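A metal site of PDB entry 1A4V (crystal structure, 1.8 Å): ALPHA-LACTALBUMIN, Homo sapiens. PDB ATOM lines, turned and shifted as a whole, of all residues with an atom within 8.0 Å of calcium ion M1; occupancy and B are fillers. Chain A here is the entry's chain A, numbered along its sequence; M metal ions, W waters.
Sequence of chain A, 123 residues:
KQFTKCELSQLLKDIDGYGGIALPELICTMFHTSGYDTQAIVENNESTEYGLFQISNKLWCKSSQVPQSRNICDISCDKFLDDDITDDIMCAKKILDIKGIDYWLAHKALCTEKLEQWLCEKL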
ATOM      1  N   THR A  38     -10.951  21.127  17.378  1.00  0.00           N
ATOM      2  CA  THR A  38      -9.788  20.836  16.501  1.00  0.00           C
ATOM      3  C   THR A  38      -8.664  21.871  16.641  1.00  0.00           C
ATOM      4  O   THR A  38      -7.556  21.653  16.147  1.00  0.00           O
ATOM      5  CB  THR A  38     -10.180  20.788  15.014  1.00  0.00           C
ATOM      6  OG1 THR A  38     -10.583  22.085  14.563  1.00  0.00           O
ATOM      7  CG2 THR A  38     -11.316  19.803  14.795  1.00  0.00           C
ATOM      8  N   ILE A  75       4.649  13.948  10.551  1.00  0.00           N
ATOM      9  CA  ILE A  75       3.753  15.013  10.132  1.00  0.00           C
ATOM     10  C   ILE A  75       4.002  16.250  11.001  1.00  0.00           C
ATOM     11  O   ILE A  75       4.480  16.123  12.124  1.00  0.00           O
ATOM     12  CB  ILE A  75       2.293  14.515  10.245  1.00  0.00           C
ATOM     13  CG1 ILE A  75       1.287  15.476   9.577  1.00  0.00           C
ATOM     14  CG2 ILE A  75       1.938  14.226  11.725  1.00  0.00           C
ATOM     15  CD1 ILE A  75      -0.155  14.897   9.461  1.00  0.00           C
ATOM     16  N   SER A  76       3.837  17.430  10.449  1.00  0.00           N
ATOM     17  CA  SER A  76       4.063  18.584  11.263  1.00  0.00           C
ATOM     18  C   SER A  76       2.782  18.834  12.076  1.00  0.00           C
ATOM     19  O   SER A  76       1.666  18.549  11.635  1.00  0.00           O
ATOM     20  CB  SER A  76       4.497  19.796  10.463  1.00  0.00           C
ATOM     21  OG  SER A  76       3.535  20.190   9.520  1.00  0.00           O
ATOM     22  N   CYS A  77       2.980  19.378  13.279  1.00  0.00           N
ATOM     23  CA  CYS A  77       1.902  19.617  14.205  1.00  0.00           C
ATOM     24  C   CYS A  77       0.804  20.550  13.736  1.00  0.00           C
ATOM     25  O   CYS A  77      -0.329  20.428  14.211  1.00  0.00           O
ATOM     26  CB  CYS A  77       2.461  20.057  15.545  1.00  0.00           C
ATOM     27  SG  CYS A  77       3.741  18.992  16.265  1.00  0.00           S
ATOM     28  N   ASP A  78       1.080  21.429  12.749  1.00  0.00           N
ATOM     29  CA  ASP A  78       0.025  22.347  12.278  1.00  0.00           C
ATOM     30  C   ASP A  78      -1.169  21.556  11.636  1.00  0.00           C
ATOM     31  O   ASP A  78      -2.280  22.043  11.566  1.00  0.00           O
ATOM     32  CB  ASP A  78       0.586  23.433  11.335  1.00  0.00           C
ATOM     33  CG  ASP A  78       1.157  22.866  10.014  1.00  0.00           C
ATOM     34  OD1 ASP A  78       2.346  22.484   9.987  1.00  0.00           O
ATOM     35  OD2 ASP A  78       0.407  22.751   9.023  1.00  0.00           O
ATOM     36  N   LYS A  79      -0.876  20.368  11.110  1.00  0.00           N
ATOM     37  CA  LYS A  79      -1.903  19.539  10.461  1.00  0.00           C
ATOM     38  C   LYS A  79      -2.944  19.023  11.442  1.00  0.00           C
ATOM     39  O   LYS A  79      -3.911  18.401  11.037  1.00  0.00           O
ATOM     40  CB  LYS A  79      -1.305  18.351   9.723  1.00  0.00           C
ATOM     41  CG  LYS A  79      -0.568  18.700   8.462  1.00  0.00           C
ATOM     42  CD  LYS A  79      -1.502  18.837   7.292  1.00  0.00           C
ATOM     43  CE  LYS A  79      -0.636  19.089   6.060  1.00  0.00           C
ATOM     44  NZ  LYS A  79      -1.513  19.531   4.988  1.00  0.00           N
ATOM     45  N   PHE A  80      -2.704  19.229  12.725  1.00  0.00           N
ATOM     46  CA  PHE A  80      -3.645  18.780  13.731  1.00  0.00           C
ATOM     47  C   PHE A  80      -4.556  19.926  14.176  1.00  0.00           C
ATOM     48  O   PHE A  80      -5.333  19.762  15.127  1.00  0.00           O
ATOM     49  CB  PHE A  80      -2.888  18.240  14.947  1.00  0.00           C
ATOM     50  CG  PHE A  80      -2.180  16.958  14.673  1.00  0.00           C
ATOM     51  CD1 PHE A  80      -2.579  16.120  13.629  1.00  0.00           C
ATOM     52  CD2 PHE A  80      -1.079  16.602  15.433  1.00  0.00           C
ATOM     53  CE1 PHE A  80      -1.885  14.969  13.305  1.00  0.00           C
ATOM     54  CE2 PHE A  80      -0.350  15.447  15.140  1.00  0.00           C
ATOM     55  CZ  PHE A  80      -0.753  14.631  14.076  1.00  0.00           C
ATOM     56  N   LEU A  81      -4.379  21.103  13.573  1.00  0.00           N
ATOM     57  CA  LEU A  81      -5.156  22.329  13.902  1.00  0.00           C
ATOM     58  C   LEU A  81      -6.202  22.739  12.892  1.00  0.00           C
ATOM     59  O   LEU A  81      -7.063  23.567  13.202  1.00  0.00           O
ATOM     60  CB  LEU A  81      -4.228  23.525  14.164  1.00  0.00           C
ATOM     61  CG  LEU A  81      -3.157  23.297  15.240  1.00  0.00           C
ATOM     62  CD1 LEU A  81      -2.212  24.486  15.371  1.00  0.00           C
ATOM     63  CD2 LEU A  81      -3.841  23.040  16.587  1.00  0.00           C
ATOM     64  N   ASP A  82      -6.187  22.075  11.724  1.00  0.00           N
ATOM     65  CA  ASP A  82      -7.148  22.306  10.653  1.00  0.00           C
ATOM     66  C   ASP A  82      -8.496  21.531  10.852  1.00  0.00           C
ATOM     67  O   ASP A  82      -8.671  20.809  11.813  1.00  0.00           O
ATOM     68  CB  ASP A  82      -6.512  22.041   9.271  1.00  0.00           C
ATOM     69  CG  ASP A  82      -6.121  20.554   9.029  1.00  0.00           C
ATOM     70  OD1 ASP A  82      -6.690  19.693   9.700  1.00  0.00           O
ATOM     71  OD2 ASP A  82      -5.255  20.268   8.159  1.00  0.00           O
ATOM     72  N   ASP A  83      -9.441  21.683   9.948  1.00  0.00           N
ATOM     73  CA  ASP A  83     -10.725  21.029  10.104  1.00  0.00           C
ATOM     74  C   ASP A  83     -10.780  19.555   9.798  1.00  0.00           C
ATOM     75  O   ASP A  83     -11.724  18.885  10.251  1.00  0.00           O
ATOM     76  CB  ASP A  83     -11.784  21.710   9.251  1.00  0.00           C
ATOM     77  CG  ASP A  83     -12.028  23.152   9.603  1.00  0.00           C
ATOM     78  OD1 ASP A  83     -11.518  23.646  10.622  1.00  0.00           O
ATOM     79  OD2 ASP A  83     -12.762  23.784   8.818  1.00  0.00           O
ATOM     80  N   ASP A  84      -9.824  19.046   8.991  1.00  0.00           N
ATOM     81  CA  ASP A  84      -9.783  17.614   8.608  1.00  0.00           C
ATOM     82  C   ASP A  84      -9.114  16.729   9.686  1.00  0.00           C
ATOM     83  O   ASP A  84      -7.921  16.819   9.870  1.00  0.00           O
ATOM     84  CB  ASP A  84      -9.050  17.474   7.308  1.00  0.00           C
ATOM     85  CG  ASP A  84      -9.133  16.075   6.745  1.00  0.00           C
ATOM     86  OD1 ASP A  84      -9.895  15.282   7.297  1.00  0.00           O
ATOM     87  OD2 ASP A  84      -8.466  15.750   5.742  1.00  0.00           O
ATOM     88  N   ILE A  85      -9.888  15.959  10.460  1.00  0.00           N
ATOM     89  CA  ILE A  85      -9.320  15.091  11.508  1.00  0.00           C
ATOM     90  C   ILE A  85      -8.836  13.716  10.980  1.00  0.00           C
ATOM     91  O   ILE A  85      -8.400  12.849  11.742  1.00  0.00           O
ATOM     92  CB  ILE A  85     -10.291  14.928  12.758  1.00  0.00           C
ATOM     93  CG1 ILE A  85     -11.594  14.230  12.343  1.00  0.00           C
ATOM     94  CG2 ILE A  85     -10.597  16.313  13.401  1.00  0.00           C
ATOM     95  CD1 ILE A  85     -12.509  13.954  13.460  1.00  0.00           C
ATOM     96  N   THR A  86      -8.832  13.546   9.668  1.00  0.00           N
ATOM     97  CA  THR A  86      -8.411  12.254   9.111  1.00  0.00           C
ATOM     98  C   THR A  86      -6.993  11.888   9.535  1.00  0.00           C
ATOM     99  O   THR A  86      -6.738  10.793  10.050  1.00  0.00           O
ATOM    100  CB  THR A  86      -8.631  12.142   7.543  1.00  0.00           C
ATOM    101  OG1 THR A  86     -10.023  12.313   7.198  1.00  0.00           O
ATOM    102  CG2 THR A  86      -8.185  10.738   7.035  1.00  0.00           C
ATOM    103  N   ASP A  87      -6.062  12.806   9.293  1.00  0.00           N
ATOM    104  CA  ASP A  87      -4.720  12.594   9.696  1.00  0.00           C
ATOM    105  C   ASP A  87      -4.481  12.540  11.202  1.00  0.00           C
ATOM    106  O   ASP A  87      -3.626  11.798  11.657  1.00  0.00           O
ATOM    107  CB  ASP A  87      -3.770  13.509   8.937  1.00  0.00           C
ATOM    108  CG  ASP A  87      -4.030  14.999   9.137  1.00  0.00           C
ATOM    109  OD1 ASP A  87      -4.724  15.369  10.064  1.00  0.00           O
ATOM    110  OD2 ASP A  87      -3.503  15.801   8.347  1.00  0.00           O
ATOM    111  N   ASP A  88      -5.292  13.238  11.981  1.00  0.00           N
ATOM    112  CA  ASP A  88      -5.222  13.215  13.434  1.00  0.00           C
ATOM    113  C   ASP A  88      -5.565  11.748  13.867  1.00  0.00           C
ATOM    114  O   ASP A  88      -4.965  11.208  14.795  1.00  0.00           O
ATOM    115  CB  ASP A  88      -6.320  14.157  14.033  1.00  0.00           C
ATOM    116  CG  ASP A  88      -6.153  15.606  13.636  1.00  0.00           C
ATOM    117  OD1 ASP A  88      -6.080  15.865  12.446  1.00  0.00           O
ATOM    118  OD2 ASP A  88      -6.082  16.500  14.492  1.00  0.00           O
ATOM    119  N   ILE A  89      -6.599  11.164  13.245  1.00  0.00           N
ATOM    120  CA  ILE A  89      -7.019   9.799  13.539  1.00  0.00           C
ATOM    121  C   ILE A  89      -5.888   8.813  13.196  1.00  0.00           C
ATOM    122  O   ILE A  89      -5.598   7.871  13.940  1.00  0.00           O
ATOM    123  CB  ILE A  89      -8.315   9.446  12.747  1.00  0.00           C
ATOM    124  CG1 ILE A  89      -9.486  10.334  13.164  1.00  0.00           C
ATOM    125  CG2 ILE A  89      -8.711   8.000  12.967  1.00  0.00           C
ATOM    126  CD1 ILE A  89     -10.707  10.009  12.350  1.00  0.00           C
HETATM  127 CA    CA M   1      -5.938  17.489  10.526  1.00  0.00          CA
HETATM  128 CA    CA M   2      -9.766  23.957  12.836  1.00  0.00          CA
HETATM  129  O   HOH W   1      -5.316  17.601   8.105  1.00  0.00           O
HETATM  130  O   HOH W   2      -7.045  18.635  12.523  1.00  0.00           O
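Water W1 lies within hydrogen-bond range of OD2 of Asp 87 (2.6 Å) and OD2 of Asp 82 (2.7 Å).
The side-chain carboxylate (OD1) of Asp 84 is in hydrogen-bond range of the side-chain hydroxyl (OG1) of Thr 86 (3.0 Å).
Of the 16 residues printed, 5 come within 4 Å of calcium ion M1.
The nearest printed residue that does not touch calcium ion M1 is Phe 80 (4.1 Å).
Calcium ion M1 is bound by the backbone carbonyl oxygen (O) of Asp 84 (2.2 Å).
O of Lys 79 is bound to calcium ion M1 (2.3 Å).
OD1 of Asp 82 binds calcium ion M1, at 2.5 Å.
OD1 of Asp 87 binds calcium ion M1.
Calcium ion M1 is bound by water W1 (2.5 Å).
Calcium ion M1 is bound by OD1 of Asp 88 (2.5 Å).
Water W2 is bound to calcium ion M1 (2.6 Å).
Calcium ion M1 has seven donor atoms within binding distance.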
